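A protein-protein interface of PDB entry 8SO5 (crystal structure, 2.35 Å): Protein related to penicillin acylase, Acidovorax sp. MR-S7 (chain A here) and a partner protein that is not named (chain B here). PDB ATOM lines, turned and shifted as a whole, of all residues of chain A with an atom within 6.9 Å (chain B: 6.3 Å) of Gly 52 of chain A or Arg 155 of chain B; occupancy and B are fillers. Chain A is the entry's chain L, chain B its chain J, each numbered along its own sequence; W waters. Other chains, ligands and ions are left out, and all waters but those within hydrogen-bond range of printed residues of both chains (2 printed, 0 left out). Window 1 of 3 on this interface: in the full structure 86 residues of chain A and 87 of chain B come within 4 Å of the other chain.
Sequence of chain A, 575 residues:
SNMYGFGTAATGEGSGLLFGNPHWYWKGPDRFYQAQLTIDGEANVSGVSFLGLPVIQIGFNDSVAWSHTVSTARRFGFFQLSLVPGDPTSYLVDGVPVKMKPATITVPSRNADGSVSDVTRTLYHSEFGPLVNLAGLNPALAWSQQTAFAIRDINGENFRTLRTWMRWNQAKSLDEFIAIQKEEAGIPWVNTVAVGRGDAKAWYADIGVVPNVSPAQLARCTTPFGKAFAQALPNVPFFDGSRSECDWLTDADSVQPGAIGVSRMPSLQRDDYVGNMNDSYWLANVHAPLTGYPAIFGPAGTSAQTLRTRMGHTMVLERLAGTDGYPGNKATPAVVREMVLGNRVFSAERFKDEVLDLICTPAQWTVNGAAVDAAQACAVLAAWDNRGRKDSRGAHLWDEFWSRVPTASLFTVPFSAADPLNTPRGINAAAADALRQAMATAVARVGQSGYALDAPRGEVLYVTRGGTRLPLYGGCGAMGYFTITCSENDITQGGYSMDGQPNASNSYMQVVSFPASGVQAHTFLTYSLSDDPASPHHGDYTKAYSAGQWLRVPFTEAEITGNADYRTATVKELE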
ATOM      1  N   GLY A  28      -2.225 -28.377 -18.892  1.00  0.00           N
ATOM      2  CA  GLY A  28      -0.953 -27.685 -18.783  1.00  0.00           C
ATOM      3  C   GLY A  28      -0.995 -26.312 -19.447  1.00  0.00           C
ATOM      4  O   GLY A  28      -1.971 -25.960 -20.106  1.00  0.00           O
ATOM      5  N   PRO A  29       0.078 -25.506 -19.298  1.00  0.00           N
ATOM      6  CA  PRO A  29       0.073 -24.116 -19.757  1.00  0.00           C
ATOM      7  C   PRO A  29       0.134 -23.943 -21.272  1.00  0.00           C
ATOM      8  O   PRO A  29      -0.077 -22.845 -21.779  1.00  0.00           O
ATOM      9  CB  PRO A  29       1.338 -23.535 -19.106  1.00  0.00           C
ATOM     10  CG  PRO A  29       2.264 -24.726 -18.959  1.00  0.00           C
ATOM     11  CD  PRO A  29       1.349 -25.896 -18.670  1.00  0.00           C
ATOM     12  N   ASP A  30       0.416 -25.037 -21.989  1.00  0.00           N
ATOM     13  CA  ASP A  30       0.573 -24.976 -23.433  1.00  0.00           C
ATOM     14  C   ASP A  30      -0.748 -25.317 -24.120  1.00  0.00           C
ATOM     15  O   ASP A  30      -0.845 -25.222 -25.341  1.00  0.00           O
ATOM     16  CB  ASP A  30       1.709 -25.887 -23.907  1.00  0.00           C
ATOM     17  CG  ASP A  30       3.102 -25.320 -23.677  1.00  0.00           C
ATOM     18  OD1 ASP A  30       3.201 -24.165 -23.215  1.00  0.00           O
ATOM     19  OD2 ASP A  30       4.081 -26.039 -23.965  1.00  0.00           O
ATOM     20  N   ARG A  31      -1.766 -25.700 -23.339  1.00  0.00           N
ATOM     21  CA  ARG A  31      -3.069 -26.008 -23.909  1.00  0.00           C
ATOM     22  C   ARG A  31      -3.666 -24.732 -24.496  1.00  0.00           C
ATOM     23  O   ARG A  31      -3.409 -23.634 -24.004  1.00  0.00           O
ATOM     24  CB  ARG A  31      -4.018 -26.627 -22.877  1.00  0.00           C
ATOM     25  CG  ARG A  31      -4.438 -25.689 -21.753  1.00  0.00           C
ATOM     26  CD  ARG A  31      -5.324 -26.378 -20.727  1.00  0.00           C
ATOM     27  NE  ARG A  31      -6.745 -26.090 -20.877  1.00  0.00           N
ATOM     28  CZ  ARG A  31      -7.713 -26.720 -20.219  1.00  0.00           C
ATOM     29  NH1 ARG A  31      -8.950 -26.259 -20.257  1.00  0.00           N
ATOM     30  NH2 ARG A  31      -7.433 -27.785 -19.486  1.00  0.00           N
ATOM     31  N   SER A  49      -5.004 -19.414 -28.361  1.00  0.00           N
ATOM     32  CA  SER A  49      -3.686 -19.051 -27.867  1.00  0.00           C
ATOM     33  C   SER A  49      -3.300 -19.989 -26.728  1.00  0.00           C
ATOM     34  O   SER A  49      -4.158 -20.412 -25.957  1.00  0.00           O
ATOM     35  CB  SER A  49      -3.660 -17.616 -27.404  1.00  0.00           C
ATOM     36  OG  SER A  49      -4.150 -16.743 -28.411  1.00  0.00           O
ATOM     37  N   PHE A  50      -2.006 -20.314 -26.632  1.00  0.00           N
ATOM     38  CA  PHE A  50      -1.480 -20.939 -25.431  1.00  0.00           C
ATOM     39  C   PHE A  50      -1.902 -20.095 -24.234  1.00  0.00           C
ATOM     40  O   PHE A  50      -1.932 -18.869 -24.325  1.00  0.00           O
ATOM     41  CB  PHE A  50       0.049 -21.022 -25.455  1.00  0.00           C
ATOM     42  CG  PHE A  50       0.658 -21.922 -26.499  1.00  0.00           C
ATOM     43  CD1 PHE A  50      -0.122 -22.761 -27.278  1.00  0.00           C
ATOM     44  CD2 PHE A  50       2.029 -21.924 -26.701  1.00  0.00           C
ATOM     45  CE1 PHE A  50       0.457 -23.583 -28.232  1.00  0.00           C
ATOM     46  CE2 PHE A  50       2.607 -22.745 -27.658  1.00  0.00           C
ATOM     47  CZ  PHE A  50       1.819 -23.572 -28.420  1.00  0.00           C
ATOM     48  N   LEU A  51      -2.225 -20.751 -23.116  1.00  0.00           N
ATOM     49  CA  LEU A  51      -2.438 -20.033 -21.873  1.00  0.00           C
ATOM     50  C   LEU A  51      -1.157 -19.274 -21.535  1.00  0.00           C
ATOM     51  O   LEU A  51      -0.089 -19.872 -21.440  1.00  0.00           O
ATOM     52  CB  LEU A  51      -2.824 -21.024 -20.769  1.00  0.00           C
ATOM     53  CG  LEU A  51      -4.280 -21.488 -20.787  1.00  0.00           C
ATOM     54  CD1 LEU A  51      -4.491 -22.643 -19.821  1.00  0.00           C
ATOM     55  CD2 LEU A  51      -5.221 -20.339 -20.452  1.00  0.00           C
ATOM     56  N   GLY A  52      -1.277 -17.951 -21.393  1.00  0.00           N
ATOM     57  CA  GLY A  52      -0.141 -17.106 -21.066  1.00  0.00           C
ATOM     58  C   GLY A  52       0.294 -16.242 -22.248  1.00  0.00           C
ATOM     59  O   GLY A  52       1.138 -15.363 -22.093  1.00  0.00           O
ATOM     60  N   LEU A  53      -0.283 -16.502 -23.426  1.00  0.00           N
ATOM     61  CA  LEU A  53       0.073 -15.766 -24.628  1.00  0.00           C
ATOM     62  C   LEU A  53      -1.046 -14.793 -24.989  1.00  0.00           C
ATOM     63  O   LEU A  53      -2.218 -15.160 -24.999  1.00  0.00           O
ATOM     64  CB  LEU A  53       0.351 -16.754 -25.764  1.00  0.00           C
ATOM     65  CG  LEU A  53       1.606 -17.605 -25.579  1.00  0.00           C
ATOM     66  CD1 LEU A  53       2.054 -18.217 -26.896  1.00  0.00           C
ATOM     67  CD2 LEU A  53       2.727 -16.781 -24.966  1.00  0.00           C
ATOM     68  N   PRO A  54      -0.701 -13.520 -25.285  1.00  0.00           N
ATOM     69  CA  PRO A  54      -1.696 -12.468 -25.500  1.00  0.00           C
ATOM     70  C   PRO A  54      -2.266 -12.302 -26.910  1.00  0.00           C
ATOM     71  O   PRO A  54      -3.175 -11.500 -27.108  1.00  0.00           O
ATOM     72  CB  PRO A  54      -0.880 -11.217 -25.145  1.00  0.00           C
ATOM     73  CG  PRO A  54       0.508 -11.542 -25.655  1.00  0.00           C
ATOM     74  CD  PRO A  54       0.680 -13.017 -25.357  1.00  0.00           C
ATOM     75  N   VAL A  55      -1.736 -13.045 -27.888  1.00  0.00           N
ATOM     76  CA  VAL A  55      -2.198 -12.906 -29.263  1.00  0.00           C
ATOM     77  C   VAL A  55      -2.634 -14.271 -29.789  1.00  0.00           C
ATOM     78  O   VAL A  55      -2.218 -15.304 -29.272  1.00  0.00           O
ATOM     79  CB  VAL A  55      -1.123 -12.280 -30.172  1.00  0.00           C
ATOM     80  CG1 VAL A  55      -0.656 -10.931 -29.647  1.00  0.00           C
ATOM     81  CG2 VAL A  55       0.059 -13.214 -30.379  1.00  0.00           C
ATOM     82  N   GLN A  57      -2.683 -17.385 -32.103  1.00  0.00           N
ATOM     83  CA  GLN A  57      -1.637 -18.106 -32.807  1.00  0.00           C
ATOM     84  C   GLN A  57      -2.254 -18.927 -33.936  1.00  0.00           C
ATOM     85  O   GLN A  57      -1.637 -19.113 -34.984  1.00  0.00           O
ATOM     86  CB  GLN A  57      -0.879 -19.004 -31.828  1.00  0.00           C
ATOM     87  CG  GLN A  57      -0.294 -18.250 -30.643  1.00  0.00           C
ATOM     88  CD  GLN A  57       0.225 -19.180 -29.574  1.00  0.00           C
ATOM     89  OE1 GLN A  57      -0.319 -19.258 -28.475  1.00  0.00           O
ATOM     90  NE2 GLN A  57       1.281 -19.907 -29.895  1.00  0.00           N
ATOM     91  N   GLN B  43      -8.590 -15.520 -19.226  1.00  0.00           N
ATOM     92  CA  GLN B  43      -7.731 -16.694 -19.216  1.00  0.00           C
ATOM     93  C   GLN B  43      -7.534 -17.180 -17.783  1.00  0.00           C
ATOM     94  O   GLN B  43      -7.629 -18.375 -17.510  1.00  0.00           O
ATOM     95  CB  GLN B  43      -6.384 -16.393 -19.874  1.00  0.00           C
ATOM     96  CG  GLN B  43      -6.381 -16.600 -21.381  1.00  0.00           C
ATOM     97  CD  GLN B  43      -4.991 -16.510 -21.963  1.00  0.00           C
ATOM     98  OE1 GLN B  43      -4.029 -17.034 -21.404  1.00  0.00           O
ATOM     99  NE2 GLN B  43      -4.872 -15.829 -23.092  1.00  0.00           N
ATOM    100  N   MET B  51      -2.315 -21.744 -14.870  1.00  0.00           N
ATOM    101  CA  MET B  51      -1.501 -20.588 -15.206  1.00  0.00           C
ATOM    102  C   MET B  51      -0.597 -20.233 -14.028  1.00  0.00           C
ATOM    103  O   MET B  51       0.595 -19.990 -14.205  1.00  0.00           O
ATOM    104  CB  MET B  51      -2.387 -19.389 -15.553  1.00  0.00           C
ATOM    105  CG  MET B  51      -2.984 -19.470 -16.945  1.00  0.00           C
ATOM    106  SD  MET B  51      -4.067 -18.070 -17.317  1.00  0.00           S
ATOM    107  CE  MET B  51      -2.879 -16.910 -17.992  1.00  0.00           C
ATOM    108  N   SER B  54       2.133 -22.435 -13.904  1.00  0.00           N
ATOM    109  CA  SER B  54       2.987 -22.262 -15.069  1.00  0.00           C
ATOM    110  C   SER B  54       4.042 -21.188 -14.809  1.00  0.00           C
ATOM    111  O   SER B  54       5.194 -21.341 -15.208  1.00  0.00           O
ATOM    112  CB  SER B  54       2.171 -21.937 -16.298  1.00  0.00           C
ATOM    113  OG  SER B  54       1.677 -20.607 -16.248  1.00  0.00           O
ATOM    114  N   PHE B  55       3.639 -20.100 -14.142  1.00  0.00           N
ATOM    115  CA  PHE B  55       4.516 -18.954 -13.958  1.00  0.00           C
ATOM    116  C   PHE B  55       5.599 -19.285 -12.934  1.00  0.00           C
ATOM    117  O   PHE B  55       6.676 -18.695 -12.961  1.00  0.00           O
ATOM    118  CB  PHE B  55       3.706 -17.708 -13.589  1.00  0.00           C
ATOM    119  CG  PHE B  55       3.017 -17.058 -14.763  1.00  0.00           C
ATOM    120  CD1 PHE B  55       3.755 -16.554 -15.822  1.00  0.00           C
ATOM    121  CD2 PHE B  55       1.636 -16.965 -14.820  1.00  0.00           C
ATOM    122  CE1 PHE B  55       3.127 -15.964 -16.908  1.00  0.00           C
ATOM    123  CE2 PHE B  55       1.009 -16.375 -15.907  1.00  0.00           C
ATOM    124  CZ  PHE B  55       1.756 -15.877 -16.948  1.00  0.00           C
ATOM    125  N   TYR B  58       8.431 -20.725 -15.289  1.00  0.00           N
ATOM    126  CA  TYR B  58       9.209 -19.827 -16.127  1.00  0.00           C
ATOM    127  C   TYR B  58      10.096 -18.944 -15.253  1.00  0.00           C
ATOM    128  O   TYR B  58      11.178 -18.544 -15.673  1.00  0.00           O
ATOM    129  CB  TYR B  58       8.277 -19.008 -17.025  1.00  0.00           C
ATOM    130  CG  TYR B  58       7.243 -19.830 -17.751  1.00  0.00           C
ATOM    131  CD1 TYR B  58       7.615 -20.890 -18.562  1.00  0.00           C
ATOM    132  CD2 TYR B  58       5.890 -19.562 -17.618  1.00  0.00           C
ATOM    133  CE1 TYR B  58       6.673 -21.658 -19.227  1.00  0.00           C
ATOM    134  CE2 TYR B  58       4.935 -20.320 -18.275  1.00  0.00           C
ATOM    135  CZ  TYR B  58       5.327 -21.373 -19.082  1.00  0.00           C
ATOM    136  OH  TYR B  58       4.389 -22.132 -19.739  1.00  0.00           O
ATOM    137  N   ILE B  94      16.306 -18.527 -19.708  1.00  0.00           N
ATOM    138  CA  ILE B  94      15.388 -17.399 -19.721  1.00  0.00           C
ATOM    139  C   ILE B  94      15.876 -16.381 -18.694  1.00  0.00           C
ATOM    140  O   ILE B  94      15.183 -16.079 -17.725  1.00  0.00           O
ATOM    141  CB  ILE B  94      13.938 -17.850 -19.455  1.00  0.00           C
ATOM    142  CG1 ILE B  94      13.545 -19.046 -20.325  1.00  0.00           C
ATOM    143  CG2 ILE B  94      12.975 -16.687 -19.631  1.00  0.00           C
ATOM    144  CD1 ILE B  94      12.081 -19.415 -20.237  1.00  0.00           C
ATOM    145  N   PHE B 117      -2.055  -7.499 -20.061  1.00  0.00           N
ATOM    146  CA  PHE B 117      -2.291  -8.910 -19.810  1.00  0.00           C
ATOM    147  C   PHE B 117      -1.990  -9.227 -18.348  1.00  0.00           C
ATOM    148  O   PHE B 117      -2.773  -9.895 -17.678  1.00  0.00           O
ATOM    149  CB  PHE B 117      -1.434  -9.772 -20.741  1.00  0.00           C
ATOM    150  CG  PHE B 117      -1.837 -11.223 -20.799  1.00  0.00           C
ATOM    151  CD1 PHE B 117      -2.871 -11.641 -21.622  1.00  0.00           C
ATOM    152  CD2 PHE B 117      -1.203 -12.168 -20.009  1.00  0.00           C
ATOM    153  CE1 PHE B 117      -3.245 -12.975 -21.671  1.00  0.00           C
ATOM    154  CE2 PHE B 117      -1.580 -13.501 -20.056  1.00  0.00           C
ATOM    155  CZ  PHE B 117      -2.600 -13.901 -20.886  1.00  0.00           C
ATOM    156  N   ARG B 150       7.224  -8.858 -17.301  1.00  0.00           N
ATOM    157  CA  ARG B 150       8.436  -9.604 -17.601  1.00  0.00           C
ATOM    158  C   ARG B 150       8.188 -11.096 -17.383  1.00  0.00           C
ATOM    159  O   ARG B 150       8.814 -11.932 -18.030  1.00  0.00           O
ATOM    160  CB  ARG B 150       9.603  -9.109 -16.738  1.00  0.00           C
ATOM    161  CG  ARG B 150      10.111  -7.725 -17.111  1.00  0.00           C
ATOM    162  CD  ARG B 150      11.157  -7.203 -16.141  1.00  0.00           C
ATOM    163  NE  ARG B 150      12.413  -7.937 -16.207  1.00  0.00           N
ATOM    164  CZ  ARG B 150      13.291  -7.843 -17.200  1.00  0.00           C
ATOM    165  NH1 ARG B 150      13.072  -7.012 -18.204  1.00  0.00           N
ATOM    166  NH2 ARG B 150      14.394  -8.572 -17.180  1.00  0.00           N
ATOM    167  N   ASP B 151       7.272 -11.416 -16.462  1.00  0.00           N
ATOM    168  CA  ASP B 151       6.895 -12.796 -16.200  1.00  0.00           C
ATOM    169  C   ASP B 151       6.199 -13.369 -17.433  1.00  0.00           C
ATOM    170  O   ASP B 151       6.425 -14.519 -17.801  1.00  0.00           O
ATOM    171  CB  ASP B 151       6.011 -12.903 -14.954  1.00  0.00           C
ATOM    172  CG  ASP B 151       6.763 -12.690 -13.652  1.00  0.00           C
ATOM    173  OD1 ASP B 151       8.010 -12.676 -13.692  1.00  0.00           O
ATOM    174  OD2 ASP B 151       6.098 -12.528 -12.610  1.00  0.00           O
ATOM    175  N   VAL B 152       5.350 -12.552 -18.064  1.00  0.00           N
ATOM    176  CA  VAL B 152       4.627 -12.975 -19.250  1.00  0.00           C
ATOM    177  C   VAL B 152       5.627 -13.151 -20.388  1.00  0.00           C
ATOM    178  O   VAL B 152       5.578 -14.139 -21.118  1.00  0.00           O
ATOM    179  CB  VAL B 152       3.516 -11.974 -19.623  1.00  0.00           C
ATOM    180  CG1 VAL B 152       2.801 -12.378 -20.904  1.00  0.00           C
ATOM    181  CG2 VAL B 152       2.520 -11.790 -18.488  1.00  0.00           C
ATOM    182  N   TRP B 153       6.543 -12.186 -20.518  1.00  0.00           N
ATOM    183  CA  TRP B 153       7.552 -12.223 -21.564  1.00  0.00           C
ATOM    184  C   TRP B 153       8.392 -13.491 -21.434  1.00  0.00           C
ATOM    185  O   TRP B 153       8.803 -14.065 -22.438  1.00  0.00           O
ATOM    186  CB  TRP B 153       8.411 -10.952 -21.539  1.00  0.00           C
ATOM    187  CG  TRP B 153       7.746  -9.781 -22.193  1.00  0.00           C
ATOM    188  CD1 TRP B 153       7.355  -8.614 -21.604  1.00  0.00           C
ATOM    189  CD2 TRP B 153       7.375  -9.671 -23.579  1.00  0.00           C
ATOM    190  NE1 TRP B 153       6.770  -7.786 -22.526  1.00  0.00           N
ATOM    191  CE2 TRP B 153       6.770  -8.408 -23.746  1.00  0.00           C
ATOM    192  CE3 TRP B 153       7.497 -10.513 -24.690  1.00  0.00           C
ATOM    193  CZ2 TRP B 153       6.289  -7.972 -24.980  1.00  0.00           C
ATOM    194  CZ3 TRP B 153       7.022 -10.080 -25.908  1.00  0.00           C
ATOM    195  CH2 TRP B 153       6.426  -8.827 -26.047  1.00  0.00           C
ATOM    196  N   ARG B 154       8.633 -13.925 -20.193  1.00  0.00           N
ATOM    197  CA  ARG B 154       9.380 -15.147 -19.948  1.00  0.00           C
ATOM    198  C   ARG B 154       8.642 -16.334 -20.564  1.00  0.00           C
ATOM    199  O   ARG B 154       9.262 -17.200 -21.175  1.00  0.00           O
ATOM    200  CB  ARG B 154       9.605 -15.351 -18.447  1.00  0.00           C
ATOM    201  CG  ARG B 154      10.711 -14.486 -17.860  1.00  0.00           C
ATOM    202  CD  ARG B 154      10.881 -14.716 -16.372  1.00  0.00           C
ATOM    203  NE  ARG B 154      11.998 -13.947 -15.843  1.00  0.00           N
ATOM    204  CZ  ARG B 154      11.874 -12.860 -15.090  1.00  0.00           C
ATOM    205  NH1 ARG B 154      10.677 -12.443 -14.715  1.00  0.00           N
ATOM    206  NH2 ARG B 154      12.952 -12.194 -14.716  1.00  0.00           N
ATOM    207  N   ARG B 155       7.314 -16.358 -20.403  1.00  0.00           N
ATOM    208  CA  ARG B 155       6.493 -17.447 -20.906  1.00  0.00           C
ATOM    209  C   ARG B 155       6.495 -17.426 -22.433  1.00  0.00           C
ATOM    210  O   ARG B 155       6.518 -18.476 -23.069  1.00  0.00           O
ATOM    211  CB  ARG B 155       5.079 -17.342 -20.321  1.00  0.00           C
ATOM    212  CG  ARG B 155       4.142 -18.474 -20.717  1.00  0.00           C
ATOM    213  CD  ARG B 155       3.353 -18.213 -21.985  1.00  0.00           C
ATOM    214  NE  ARG B 155       2.568 -19.392 -22.314  1.00  0.00           N
ATOM    215  CZ  ARG B 155       3.090 -20.571 -22.629  1.00  0.00           C
ATOM    216  NH1 ARG B 155       4.374 -20.667 -22.927  1.00  0.00           N
ATOM    217  NH2 ARG B 155       2.318 -21.643 -22.687  1.00  0.00           N
ATOM    218  N   ILE B 156       6.489 -16.218 -23.008  1.00  0.00           N
ATOM    219  CA  ILE B 156       6.486 -16.046 -24.452  1.00  0.00           C
ATOM    220  C   ILE B 156       7.807 -16.561 -25.020  1.00  0.00           C
ATOM    221  O   ILE B 156       7.817 -17.264 -26.028  1.00  0.00           O
ATOM    222  CB  ILE B 156       6.226 -14.571 -24.821  1.00  0.00           C
ATOM    223  CG1 ILE B 156       4.801 -14.147 -24.452  1.00  0.00           C
ATOM    224  CG2 ILE B 156       6.521 -14.320 -26.292  1.00  0.00           C
ATOM    225  CD1 ILE B 156       4.620 -12.656 -24.290  1.00  0.00           C
ATOM    226  N   TYR B 157       8.917 -16.205 -24.365  1.00  0.00           N
ATOM    227  CA  TYR B 157      10.232 -16.659 -24.789  1.00  0.00           C
ATOM    228  C   TYR B 157      10.290 -18.181 -24.692  1.00  0.00           C
ATOM    229  O   TYR B 157      10.860 -18.840 -25.557  1.00  0.00           O
ATOM    230  CB  TYR B 157      11.330 -16.007 -23.942  1.00  0.00           C
ATOM    231  CG  TYR B 157      12.741 -16.273 -24.405  1.00  0.00           C
ATOM    232  CD1 TYR B 157      13.252 -15.661 -25.537  1.00  0.00           C
ATOM    233  CD2 TYR B 157      13.568 -17.143 -23.713  1.00  0.00           C
ATOM    234  CE1 TYR B 157      14.548 -15.900 -25.967  1.00  0.00           C
ATOM    235  CE2 TYR B 157      14.864 -17.396 -24.130  1.00  0.00           C
ATOM    236  CZ  TYR B 157      15.357 -16.770 -25.262  1.00  0.00           C
ATOM    237  OH  TYR B 157      16.642 -17.014 -25.683  1.00  0.00           O
ATOM    238  N   ALA B 158       9.676 -18.725 -23.635  1.00  0.00           N
ATOM    239  CA  ALA B 158       9.722 -20.154 -23.368  1.00  0.00           C
ATOM    240  C   ALA B 158       9.044 -20.923 -24.500  1.00  0.00           C
ATOM    241  O   ALA B 158       9.483 -22.011 -24.864  1.00  0.00           O
ATOM    242  CB  ALA B 158       9.074 -20.452 -22.037  1.00  0.00           C
ATOM    243  N   ALA B 159       7.972 -20.343 -25.051  1.00  0.00           N
ATOM    244  CA  ALA B 159       7.192 -20.996 -26.091  1.00  0.00           C
ATOM    245  C   ALA B 159       8.037 -21.185 -27.349  1.00  0.00           C
ATOM    246  O   ALA B 159       7.777 -22.084 -28.146  1.00  0.00           O
ATOM    247  CB  ALA B 159       5.948 -20.189 -26.381  1.00  0.00           C
ATOM    248  N   ASN B 160       9.054 -20.332 -27.512  1.00  0.00           N
ATOM    249  CA  ASN B 160       9.876 -20.323 -28.711  1.00  0.00           C
ATOM    250  C   ASN B 160      10.840 -21.507 -28.722  1.00  0.00           C
ATOM    251  O   ASN B 160      11.306 -21.914 -29.784  1.00  0.00           O
ATOM    252  CB  ASN B 160      10.669 -19.021 -28.840  1.00  0.00           C
ATOM    253  CG  ASN B 160       9.918 -17.936 -29.580  1.00  0.00           C
ATOM    254  OD1 ASN B 160       8.766 -17.643 -29.265  1.00  0.00           O
ATOM    255  ND2 ASN B 160      10.560 -17.342 -30.573  1.00  0.00           N
HETATM  256  O   HOH W   1       5.732 -22.907 -23.944  1.00  0.00           O
HETATM  257  O   HOH W   2       0.027 -19.865 -18.552  1.00  0.00           O
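Among the printed residues, 15 pairs touch across the chains.
Among the printed residues, pairs that only touch across the chains: Pro 29 of chain A with Ser 54 of chain B (3.3 Å), Leu 53 of chain A with Arg 155 of chain B (3.4 Å), Leu 53 of chain A with Ile 156 of chain B (3.4 Å), Pro 29 of chain A with Tyr 58 of chain B (3.4 Å), Leu 51 of chain A with Gln 43 of chain B (3.4 Å), Gly 52 of chain A with Arg 155 of chain B (3.6 Å), Gly 52 of chain A with Val 152 of chain B (3.6 Å), Phe 50 of chain A with Arg 155 of chain B (3.6 Å), Gly 52 of chain A with Phe 117 of chain B (3.9 Å) and Gly 52 of chain A with Met 51 of chain B (3.9 Å).
Arg 155 of chain B touches just these residues of chain A: Pro 29 (2.8 Å), Asp 30 (2.7 Å), Phe 50 (3.6 Å), Leu 51 (2.8 Å), Gly 52 (3.6 Å) and Leu 53 (3.4 Å). Of the printed residues of chain B, Leu 51 of chain A touches Gln 43 and Arg 155. Of the printed residues of chain A, Tyr 58 of chain B touches Pro 29. Printed residues of chain A within 4 Å of Met 51 of chain B: Gly 52 (3.9 Å). Of the printed residues of chain A, Ile 156 of chain B touches Leu 53 (3.4 Å). Printed residues of chain A within 4 Å of Val 152 of chain B: Gly 52. Phe 55 of chain B touches none of the printed residues of chain A. Arg 154 of chain B touches none of the printed residues of chain A. The nearest residue of chain B that does not touch Gly 52 of chain A is Ile 156 of chain B (4.5 Å). The nearest printed residue of chain A that does not touch Val 152 of chain B is Pro 54 of chain A (5.0 Å).
Water W1 lies within hydrogen-bond range of NH1 of Arg 155 of chain B (2.8 Å) and OD1 of Asp 30 of chain A (2.9 Å). Water W2 lies within hydrogen-bond range of the backbone carbonyl oxygen of Leu 51 of chain A (2.9 Å) and the side-chain hydroxyl of Ser 54 of chain B (2.9 Å).
N of Gly 52 of chain A is in hydrogen-bond range of OE1 of Gln 43 of chain B, at 2.9 Å. The backbone carbonyl oxygen (O) of Leu 53 of chain A sits at hydrogen-bond distance from the side-chain amide nitrogen (NE2) of Gln 43 of chain B, 3.3 Å away. The guanidinium group (NH2) of Arg 155 of chain B lies within hydrogen-bond range of the backbone carbonyl oxygen (O) of Pro 29 of chain A, at 2.8 Å. The side-chain carboxylate (OD1) of Asp 30 of chain A lies within salt-bridge range of the guanidinium group (NH2) of Arg 155 of chain B, at 2.7 Å. NE of Arg 155 of chain B lies within hydrogen-bond range of O of Leu 51 of chain A, at 2.8 Å.
The backbone carbonyl oxygen (O) of Ile 156 of chain B sits close to the side-chain amide oxygen (OD1) of Asn 160 of chain B (3.4 Å). The backbone carbonyl oxygen of Pro 29 of chain A lies within hydrogen-bond range of the backbone NH of Leu 51 of chain A, 3.3 Å away. The backbone NH (N) of Leu 51 of chain A lies within hydrogen-bond range of the backbone carbonyl oxygen (O) of Arg 31 of chain A (3.2 Å). N of Phe 50 of chain A is in hydrogen-bond range of OE1 of Gln 57 of chain A (2.7 Å).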
